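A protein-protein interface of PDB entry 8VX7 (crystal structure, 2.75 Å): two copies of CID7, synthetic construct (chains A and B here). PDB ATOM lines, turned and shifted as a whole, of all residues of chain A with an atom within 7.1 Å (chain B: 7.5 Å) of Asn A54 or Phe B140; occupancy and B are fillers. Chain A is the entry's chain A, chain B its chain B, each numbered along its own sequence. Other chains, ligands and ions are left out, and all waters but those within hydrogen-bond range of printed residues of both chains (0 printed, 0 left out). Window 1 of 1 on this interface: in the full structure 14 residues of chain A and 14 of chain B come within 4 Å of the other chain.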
ATOM      1  N   VAL A  10     -18.733  17.762  12.726  1.00  0.00           N
ATOM      2  CA  VAL A  10     -19.807  16.865  12.315  1.00  0.00           C
ATOM      3  C   VAL A  10     -19.243  15.526  11.861  1.00  0.00           C
ATOM      4  O   VAL A  10     -19.787  14.464  12.188  1.00  0.00           O
ATOM      5  CB  VAL A  10     -20.655  17.525  11.213  1.00  0.00           C
ATOM      6  CG1 VAL A  10     -21.783  16.606  10.793  1.00  0.00           C
ATOM      7  CG2 VAL A  10     -21.208  18.854  11.700  1.00  0.00           C
ATOM      8  N   LEU A  14     -20.164  12.227  13.995  1.00  0.00           N
ATOM      9  CA  LEU A  14     -20.923  11.138  13.397  1.00  0.00           C
ATOM     10  C   LEU A  14     -20.122   9.847  13.281  1.00  0.00           C
ATOM     11  O   LEU A  14     -20.701   8.805  12.957  1.00  0.00           O
ATOM     12  CB  LEU A  14     -21.431  11.551  12.013  1.00  0.00           C
ATOM     13  N   LYS A  47     -23.464  24.094   1.603  1.00  0.00           N
ATOM     14  CA  LYS A  47     -22.755  23.100   2.400  1.00  0.00           C
ATOM     15  C   LYS A  47     -23.255  23.078   3.840  1.00  0.00           C
ATOM     16  O   LYS A  47     -23.377  22.004   4.440  1.00  0.00           O
ATOM     17  CB  LYS A  47     -21.250  23.371   2.359  1.00  0.00           C
ATOM     18  CG  LYS A  47     -20.417  22.420   3.206  1.00  0.00           C
ATOM     19  CD  LYS A  47     -20.439  21.008   2.642  1.00  0.00           C
ATOM     20  CE  LYS A  47     -19.047  20.393   2.637  1.00  0.00           C
ATOM     21  NZ  LYS A  47     -18.787  19.592   3.864  1.00  0.00           N
ATOM     22  N   ALA A  48     -23.552  24.251   4.405  1.00  0.00           N
ATOM     23  CA  ALA A  48     -24.052  24.312   5.775  1.00  0.00           C
ATOM     24  C   ALA A  48     -25.390  23.594   5.902  1.00  0.00           C
ATOM     25  O   ALA A  48     -25.592  22.789   6.819  1.00  0.00           O
ATOM     26  CB  ALA A  48     -24.175  25.767   6.226  1.00  0.00           C
ATOM     27  N   LEU A  49     -26.322  23.877   4.989  1.00  0.00           N
ATOM     28  CA  LEU A  49     -27.614  23.202   5.026  1.00  0.00           C
ATOM     29  C   LEU A  49     -27.474  21.713   4.738  1.00  0.00           C
ATOM     30  O   LEU A  49     -28.254  20.906   5.256  1.00  0.00           O
ATOM     31  CB  LEU A  49     -28.579  23.855   4.037  1.00  0.00           C
ATOM     32  CG  LEU A  49     -29.384  25.032   4.593  1.00  0.00           C
ATOM     33  CD1 LEU A  49     -29.643  26.068   3.506  1.00  0.00           C
ATOM     34  CD2 LEU A  49     -30.691  24.558   5.214  1.00  0.00           C
ATOM     35  N   GLN A  50     -26.484  21.334   3.928  1.00  0.00           N
ATOM     36  CA  GLN A  50     -26.209  19.918   3.705  1.00  0.00           C
ATOM     37  C   GLN A  50     -25.743  19.241   4.986  1.00  0.00           C
ATOM     38  O   GLN A  50     -26.146  18.110   5.284  1.00  0.00           O
ATOM     39  CB  GLN A  50     -25.166  19.762   2.598  1.00  0.00           C
ATOM     40  CG  GLN A  50     -24.261  18.557   2.749  1.00  0.00           C
ATOM     41  CD  GLN A  50     -22.945  18.735   2.024  1.00  0.00           C
ATOM     42  N   LEU A  51     -24.899  19.921   5.766  1.00  0.00           N
ATOM     43  CA  LEU A  51     -24.430  19.347   7.023  1.00  0.00           C
ATOM     44  C   LEU A  51     -25.541  19.317   8.066  1.00  0.00           C
ATOM     45  O   LEU A  51     -25.648  18.355   8.837  1.00  0.00           O
ATOM     46  CB  LEU A  51     -23.225  20.131   7.541  1.00  0.00           C
ATOM     47  CG  LEU A  51     -21.898  19.882   6.822  1.00  0.00           C
ATOM     48  CD1 LEU A  51     -20.903  20.994   7.127  1.00  0.00           C
ATOM     49  CD2 LEU A  51     -21.325  18.525   7.203  1.00  0.00           C
ATOM     50  N   ALA A  52     -26.376  20.357   8.104  1.00  0.00           N
ATOM     51  CA  ALA A  52     -27.472  20.395   9.068  1.00  0.00           C
ATOM     52  C   ALA A  52     -28.452  19.255   8.829  1.00  0.00           C
ATOM     53  O   ALA A  52     -28.895  18.591   9.773  1.00  0.00           O
ATOM     54  CB  ALA A  52     -28.189  21.742   8.994  1.00  0.00           C
ATOM     55  N   VAL A  53     -28.805  19.016   7.564  1.00  0.00           N
ATOM     56  CA  VAL A  53     -29.729  17.935   7.240  1.00  0.00           C
ATOM     57  C   VAL A  53     -29.105  16.585   7.572  1.00  0.00           C
ATOM     58  O   VAL A  53     -29.780  15.682   8.082  1.00  0.00           O
ATOM     59  CB  VAL A  53     -30.151  18.028   5.760  1.00  0.00           C
ATOM     60  CG1 VAL A  53     -30.410  16.644   5.173  1.00  0.00           C
ATOM     61  CG2 VAL A  53     -31.380  18.918   5.615  1.00  0.00           C
ATOM     62  N   ASN A  54     -27.803  16.434   7.312  1.00  0.00           N
ATOM     63  CA  ASN A  54     -27.127  15.178   7.612  1.00  0.00           C
ATOM     64  C   ASN A  54     -27.125  14.877   9.105  1.00  0.00           C
ATOM     65  O   ASN A  54     -27.184  13.708   9.500  1.00  0.00           O
ATOM     66  CB  ASN A  54     -25.697  15.209   7.072  1.00  0.00           C
ATOM     67  CG  ASN A  54     -25.604  14.712   5.642  1.00  0.00           C
ATOM     68  OD1 ASN A  54     -26.266  13.744   5.266  1.00  0.00           O
ATOM     69  ND2 ASN A  54     -24.782  15.374   4.838  1.00  0.00           N
ATOM     70  N   VAL A  55     -27.062  15.909   9.949  1.00  0.00           N
ATOM     71  CA  VAL A  55     -27.082  15.679  11.391  1.00  0.00           C
ATOM     72  C   VAL A  55     -28.485  15.290  11.843  1.00  0.00           C
ATOM     73  O   VAL A  55     -28.671  14.314  12.578  1.00  0.00           O
ATOM     74  CB  VAL A  55     -26.570  16.920  12.144  1.00  0.00           C
ATOM     75  CG1 VAL A  55     -27.124  16.954  13.567  1.00  0.00           C
ATOM     76  CG2 VAL A  55     -25.054  16.958  12.149  1.00  0.00           C
ATOM     77  N   ALA A  56     -29.495  16.041  11.394  1.00  0.00           N
ATOM     78  CA  ALA A  56     -30.870  15.760  11.798  1.00  0.00           C
ATOM     79  C   ALA A  56     -31.364  14.430  11.245  1.00  0.00           C
ATOM     80  O   ALA A  56     -32.263  13.814  11.828  1.00  0.00           O
ATOM     81  CB  ALA A  56     -31.791  16.895  11.350  1.00  0.00           C
ATOM     82  N   ASP A  57     -30.794  13.972  10.130  1.00  0.00           N
ATOM     83  CA  ASP A  57     -31.199  12.689   9.568  1.00  0.00           C
ATOM     84  C   ASP A  57     -30.752  11.526  10.447  1.00  0.00           C
ATOM     85  O   ASP A  57     -31.394  10.469  10.448  1.00  0.00           O
ATOM     86  CB  ASP A  57     -30.639  12.542   8.154  1.00  0.00           C
ATOM     87  CG  ASP A  57     -30.825  11.147   7.591  1.00  0.00           C
ATOM     88  OD1 ASP A  57     -31.988  10.719   7.435  1.00  0.00           O
ATOM     89  OD2 ASP A  57     -29.808  10.483   7.302  1.00  0.00           O
ATOM     90  N   HIS A  58     -29.675  11.705  11.209  1.00  0.00           N
ATOM     91  CA  HIS A  58     -29.108  10.621  12.003  1.00  0.00           C
ATOM     92  C   HIS A  58     -29.642  10.611  13.433  1.00  0.00           C
ATOM     93  O   HIS A  58     -30.073   9.564  13.928  1.00  0.00           O
ATOM     94  CB  HIS A  58     -27.579  10.720  12.001  1.00  0.00           C
ATOM     95  CG  HIS A  58     -26.933  10.179  13.238  1.00  0.00           C
ATOM     96  ND1 HIS A  58     -26.690  10.953  14.353  1.00  0.00           N
ATOM     97  CD2 HIS A  58     -26.477   8.939  13.536  1.00  0.00           C
ATOM     98  CE1 HIS A  58     -26.116  10.213  15.285  1.00  0.00           C
ATOM     99  NE2 HIS A  58     -25.975   8.987  14.814  1.00  0.00           N
ATOM    100  N   ASN A  59     -29.624  11.759  14.107  1.00  0.00           N
ATOM    101  CA  ASN A  59     -30.062  11.843  15.494  1.00  0.00           C
ATOM    102  C   ASN A  59     -31.496  12.338  15.654  1.00  0.00           C
ATOM    103  O   ASN A  59     -31.989  12.404  16.784  1.00  0.00           O
ATOM    104  CB  ASN A  59     -29.095  12.725  16.304  1.00  0.00           C
ATOM    105  CG  ASN A  59     -29.234  14.215  15.999  1.00  0.00           C
ATOM    106  OD1 ASN A  59     -29.982  14.625  15.110  1.00  0.00           O
ATOM    107  ND2 ASN A  59     -28.503  15.033  16.748  1.00  0.00           N
ATOM    108  N   LEU A  64     -32.907  21.419  15.202  1.00  0.00           N
ATOM    109  CA  LEU A  64     -32.034  21.787  14.094  1.00  0.00           C
ATOM    110  C   LEU A  64     -32.741  21.631  12.754  1.00  0.00           C
ATOM    111  O   LEU A  64     -32.467  22.384  11.813  1.00  0.00           O
ATOM    112  CB  LEU A  64     -30.762  20.938  14.125  1.00  0.00           C
ATOM    113  CG  LEU A  64     -29.711  21.242  13.058  1.00  0.00           C
ATOM    114  CD1 LEU A  64     -28.966  22.530  13.386  1.00  0.00           C
ATOM    115  CD2 LEU A  64     -28.750  20.075  12.904  1.00  0.00           C
ATOM    116  N   TRP A  97     -37.020  18.005   0.833  1.00  0.00           N
ATOM    117  CA  TRP A  97     -36.592  16.952   1.749  1.00  0.00           C
ATOM    118  C   TRP A  97     -36.939  17.307   3.190  1.00  0.00           C
ATOM    119  O   TRP A  97     -37.453  16.470   3.941  1.00  0.00           O
ATOM    120  CB  TRP A  97     -35.091  16.697   1.601  1.00  0.00           C
ATOM    121  CG  TRP A  97     -34.625  15.492   2.359  1.00  0.00           C
ATOM    122  CD1 TRP A  97     -34.469  14.226   1.872  1.00  0.00           C
ATOM    123  CD2 TRP A  97     -34.267  15.433   3.746  1.00  0.00           C
ATOM    124  NE1 TRP A  97     -34.032  13.385   2.867  1.00  0.00           N
ATOM    125  CE2 TRP A  97     -33.901  14.101   4.027  1.00  0.00           C
ATOM    126  CE3 TRP A  97     -34.217  16.378   4.776  1.00  0.00           C
ATOM    127  CZ2 TRP A  97     -33.491  13.690   5.294  1.00  0.00           C
ATOM    128  CZ3 TRP A  97     -33.811  15.967   6.035  1.00  0.00           C
ATOM    129  CH2 TRP A  97     -33.453  14.635   6.283  1.00  0.00           C
ATOM    130  N   LEU B  96     -26.345   4.075  -1.402  1.00  0.00           N
ATOM    131  CA  LEU B  96     -26.613   4.204   0.026  1.00  0.00           C
ATOM    132  C   LEU B  96     -28.060   4.605   0.290  1.00  0.00           C
ATOM    133  O   LEU B  96     -28.600   4.302   1.360  1.00  0.00           O
ATOM    134  CB  LEU B  96     -25.653   5.220   0.643  1.00  0.00           C
ATOM    135  CG  LEU B  96     -25.652   5.398   2.164  1.00  0.00           C
ATOM    136  CD1 LEU B  96     -25.328   4.089   2.863  1.00  0.00           C
ATOM    137  CD2 LEU B  96     -24.671   6.485   2.571  1.00  0.00           C
ATOM    138  N   TYR B 108     -25.235  -2.850   1.074  1.00  0.00           N
ATOM    139  CA  TYR B 108     -24.336  -2.269   2.064  1.00  0.00           C
ATOM    140  C   TYR B 108     -22.972  -2.949   2.039  1.00  0.00           C
ATOM    141  O   TYR B 108     -21.938  -2.282   2.158  1.00  0.00           O
ATOM    142  CB  TYR B 108     -24.956  -2.364   3.459  1.00  0.00           C
ATOM    143  CG  TYR B 108     -25.408  -1.038   4.029  1.00  0.00           C
ATOM    144  CD1 TYR B 108     -24.487  -0.068   4.402  1.00  0.00           C
ATOM    145  CD2 TYR B 108     -26.757  -0.761   4.207  1.00  0.00           C
ATOM    146  CE1 TYR B 108     -24.896   1.143   4.929  1.00  0.00           C
ATOM    147  CE2 TYR B 108     -27.177   0.447   4.733  1.00  0.00           C
ATOM    148  CZ  TYR B 108     -26.243   1.395   5.092  1.00  0.00           C
ATOM    149  OH  TYR B 108     -26.657   2.598   5.613  1.00  0.00           O
ATOM    150  N   ILE B 133     -17.467  15.162   0.913  1.00  0.00           N
ATOM    151  CA  ILE B 133     -18.735  14.460   0.735  1.00  0.00           C
ATOM    152  C   ILE B 133     -18.503  12.957   0.741  1.00  0.00           C
ATOM    153  O   ILE B 133     -19.277  12.190   1.329  1.00  0.00           O
ATOM    154  CB  ILE B 133     -19.416  14.925  -0.566  1.00  0.00           C
ATOM    155  CG1 ILE B 133     -20.059  16.299  -0.371  1.00  0.00           C
ATOM    156  CG2 ILE B 133     -20.447  13.904  -1.040  1.00  0.00           C
ATOM    157  CD1 ILE B 133     -21.332  16.255   0.435  1.00  0.00           C
ATOM    158  N   LEU B 134     -17.418  12.516   0.102  1.00  0.00           N
ATOM    159  CA  LEU B 134     -17.121  11.093   0.006  1.00  0.00           C
ATOM    160  C   LEU B 134     -16.754  10.506   1.365  1.00  0.00           C
ATOM    161  O   LEU B 134     -17.089   9.353   1.659  1.00  0.00           O
ATOM    162  CB  LEU B 134     -15.991  10.881  -0.998  1.00  0.00           C
ATOM    163  CG  LEU B 134     -16.385  10.513  -2.428  1.00  0.00           C
ATOM    164  CD1 LEU B 134     -15.241   9.789  -3.100  1.00  0.00           C
ATOM    165  CD2 LEU B 134     -17.638   9.654  -2.437  1.00  0.00           C
ATOM    166  N   ILE B 135     -16.061  11.283   2.203  1.00  0.00           N
ATOM    167  CA  ILE B 135     -15.730  10.819   3.547  1.00  0.00           C
ATOM    168  C   ILE B 135     -17.001  10.600   4.356  1.00  0.00           C
ATOM    169  O   ILE B 135     -17.154   9.587   5.048  1.00  0.00           O
ATOM    170  CB  ILE B 135     -14.780  11.812   4.242  1.00  0.00           C
ATOM    171  CG1 ILE B 135     -13.331  11.540   3.833  1.00  0.00           C
ATOM    172  CG2 ILE B 135     -14.920  11.731   5.758  1.00  0.00           C
ATOM    173  CD1 ILE B 135     -12.699  10.382   4.566  1.00  0.00           C
ATOM    174  N   LEU B 136     -17.939  11.550   4.272  1.00  0.00           N
ATOM    175  CA  LEU B 136     -19.217  11.391   4.956  1.00  0.00           C
ATOM    176  C   LEU B 136     -19.945  10.143   4.477  1.00  0.00           C
ATOM    177  O   LEU B 136     -20.609   9.459   5.267  1.00  0.00           O
ATOM    178  CB  LEU B 136     -20.080  12.636   4.749  1.00  0.00           C
ATOM    179  CG  LEU B 136     -21.278  12.799   5.690  1.00  0.00           C
ATOM    180  CD1 LEU B 136     -20.937  12.318   7.092  1.00  0.00           C
ATOM    181  CD2 LEU B 136     -21.747  14.245   5.716  1.00  0.00           C
ATOM    182  N   LEU B 137     -19.825   9.823   3.185  1.00  0.00           N
ATOM    183  CA  LEU B 137     -20.377   8.573   2.676  1.00  0.00           C
ATOM    184  C   LEU B 137     -19.717   7.367   3.329  1.00  0.00           C
ATOM    185  O   LEU B 137     -20.371   6.340   3.541  1.00  0.00           O
ATOM    186  CB  LEU B 137     -20.214   8.506   1.156  1.00  0.00           C
ATOM    187  CG  LEU B 137     -21.388   7.940   0.356  1.00  0.00           C
ATOM    188  N   GLY B 138     -18.428   7.472   3.659  1.00  0.00           N
ATOM    189  CA  GLY B 138     -17.739   6.363   4.293  1.00  0.00           C
ATOM    190  C   GLY B 138     -18.151   6.140   5.734  1.00  0.00           C
ATOM    191  O   GLY B 138     -18.163   5.000   6.207  1.00  0.00           O
ATOM    192  N   ILE B 139     -18.489   7.213   6.453  1.00  0.00           N
ATOM    193  CA  ILE B 139     -18.906   7.067   7.845  1.00  0.00           C
ATOM    194  C   ILE B 139     -20.239   6.334   7.930  1.00  0.00           C
ATOM    195  O   ILE B 139     -20.393   5.382   8.704  1.00  0.00           O
ATOM    196  CB  ILE B 139     -18.970   8.437   8.548  1.00  0.00           C
ATOM    197  CG1 ILE B 139     -17.601   9.124   8.535  1.00  0.00           C
ATOM    198  CG2 ILE B 139     -19.483   8.284   9.970  1.00  0.00           C
ATOM    199  CD1 ILE B 139     -17.638  10.564   8.073  1.00  0.00           C
ATOM    200  N   PHE B 140     -21.222   6.765   7.135  1.00  0.00           N
ATOM    201  CA  PHE B 140     -22.516   6.089   7.129  1.00  0.00           C
ATOM    202  C   PHE B 140     -22.382   4.632   6.709  1.00  0.00           C
ATOM    203  O   PHE B 140     -23.119   3.771   7.205  1.00  0.00           O
ATOM    204  CB  PHE B 140     -23.487   6.824   6.204  1.00  0.00           C
ATOM    205  CG  PHE B 140     -23.765   8.242   6.621  1.00  0.00           C
ATOM    206  CD1 PHE B 140     -23.995   8.555   7.951  1.00  0.00           C
ATOM    207  CD2 PHE B 140     -23.791   9.262   5.683  1.00  0.00           C
ATOM    208  CE1 PHE B 140     -24.248   9.859   8.338  1.00  0.00           C
ATOM    209  CE2 PHE B 140     -24.044  10.567   6.064  1.00  0.00           C
ATOM    210  CZ  PHE B 140     -24.273  10.865   7.393  1.00  0.00           C
ATOM    211  N   ILE B 141     -21.447   4.335   5.804  1.00  0.00           N
ATOM    212  CA  ILE B 141     -21.199   2.950   5.413  1.00  0.00           C
ATOM    213  C   ILE B 141     -20.669   2.156   6.600  1.00  0.00           C
ATOM    214  O   ILE B 141     -21.134   1.047   6.889  1.00  0.00           O
ATOM    215  CB  ILE B 141     -20.229   2.898   4.218  1.00  0.00           C
ATOM    216  CG1 ILE B 141     -20.968   3.208   2.916  1.00  0.00           C
ATOM    217  CG2 ILE B 141     -19.545   1.540   4.139  1.00  0.00           C
ATOM    218  CD1 ILE B 141     -20.049   3.459   1.742  1.00  0.00           C
ATOM    219  N   ALA B 142     -19.694   2.720   7.315  1.00  0.00           N
ATOM    220  CA  ALA B 142     -19.081   2.008   8.429  1.00  0.00           C
ATOM    221  C   ALA B 142     -19.948   2.020   9.681  1.00  0.00           C
ATOM    222  O   ALA B 142     -19.856   1.097  10.498  1.00  0.00           O
ATOM    223  CB  ALA B 142     -17.709   2.608   8.739  1.00  0.00           C
ATOM    224  N   ARG B 143     -20.792   3.040   9.854  1.00  0.00           N
ATOM    225  CA  ARG B 143     -21.593   3.129  11.071  1.00  0.00           C
ATOM    226  C   ARG B 143     -22.885   2.331  10.949  1.00  0.00           C
ATOM    227  O   ARG B 143     -23.215   1.534  11.835  1.00  0.00           O
ATOM    228  CB  ARG B 143     -21.895   4.594  11.397  1.00  0.00           C
ATOM    229  N   ASP B 144     -23.630   2.530   9.861  1.00  0.00           N
ATOM    230  CA  ASP B 144     -24.926   1.880   9.715  1.00  0.00           C
ATOM    231  C   ASP B 144     -24.815   0.403   9.362  1.00  0.00           C
ATOM    232  O   ASP B 144     -25.744  -0.358   9.654  1.00  0.00           O
ATOM    233  CB  ASP B 144     -25.760   2.606   8.658  1.00  0.00           C
ATOM    234  CG  ASP B 144     -26.046   4.049   9.030  1.00  0.00           C
ATOM    235  OD1 ASP B 144     -25.908   4.395  10.222  1.00  0.00           O
ATOM    236  OD2 ASP B 144     -26.409   4.837   8.132  1.00  0.00           O
ATOM    237  N   ALA B 145     -23.713  -0.022   8.746  1.00  0.00           N
ATOM    238  CA  ALA B 145     -23.514  -1.426   8.412  1.00  0.00           C
ATOM    239  C   ALA B 145     -22.674  -2.173   9.437  1.00  0.00           C
ATOM    240  O   ALA B 145     -22.572  -3.403   9.350  1.00  0.00           O
ATOM    241  CB  ALA B 145     -22.861  -1.564   7.033  1.00  0.00           C
ATOM    242  N   GLY B 146     -22.075  -1.472  10.396  1.00  0.00           N
ATOM    243  CA  GLY B 146     -21.237  -2.115  11.387  1.00  0.00           C
ATOM    244  C   GLY B 146     -20.004  -2.755  10.785  1.00  0.00           C
ATOM    245  O   GLY B 146     -19.818  -3.971  10.877  1.00  0.00           O
ATOM    246  N   VAL B 154     -11.997   5.237   7.322  1.00  0.00           N
ATOM    247  CA  VAL B 154     -12.510   6.601   7.221  1.00  0.00           C
ATOM    248  C   VAL B 154     -11.952   7.471   8.338  1.00  0.00           C
ATOM    249  O   VAL B 154     -11.797   8.687   8.168  1.00  0.00           O
ATOM    250  CB  VAL B 154     -14.050   6.597   7.223  1.00  0.00           C
ATOM    251  CG1 VAL B 154     -14.582   7.885   6.619  1.00  0.00           C
ATOM    252  CG2 VAL B 154     -14.575   5.405   6.444  1.00  0.00           C
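Of the 17 printed residues of chain B, 4 touch a printed residue of chain A. Hydrophobic or aromatic side chains of chain B within 4 Å of the printed part of chain A: Ile B133, Leu B136, Ile B139 and Phe B140. Along chain B the printed residues that touch a printed residue of chain A span positions 133 to 140. Among the printed residues, 4 pairs touch across the chains.
No position is printed for both chains. Of the 4 pairs that touch across the chains among the printed residues, none has its exchanged pair printed and touching as well.
Printed residues of chain B within 4 Å of Leu A14: Ile B139 (3.3 Å). Of the printed residues of chain B, Gln A50 touches Ile B133. Of the printed residues of chain A, Ile B133 touches Gln A50. Of the printed residues of chain A, Leu B136 touches Asn A54. Printed residues of chain A within 4 Å of Ile B139: Leu A14 (3.3 Å). Phe B140 touches just one residue of chain A: Asn A54 (3.96 Å). The nearest residue of chain B that does not touch Asn A54 is Ile B133 (5.7 Å).
Among the printed residues, pairs that only touch across the chains: Leu A14 with Ile B139 (3.3 Å), Asn A54 with Leu B136 (3.4 Å), Gln A50 with Ile B133 (3.4 Å) and Asn A54 with Phe B140 (3.96 Å).
O of Gln A50 is in hydrogen-bond range of ND2 of Asn A54 (3.1 Å).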
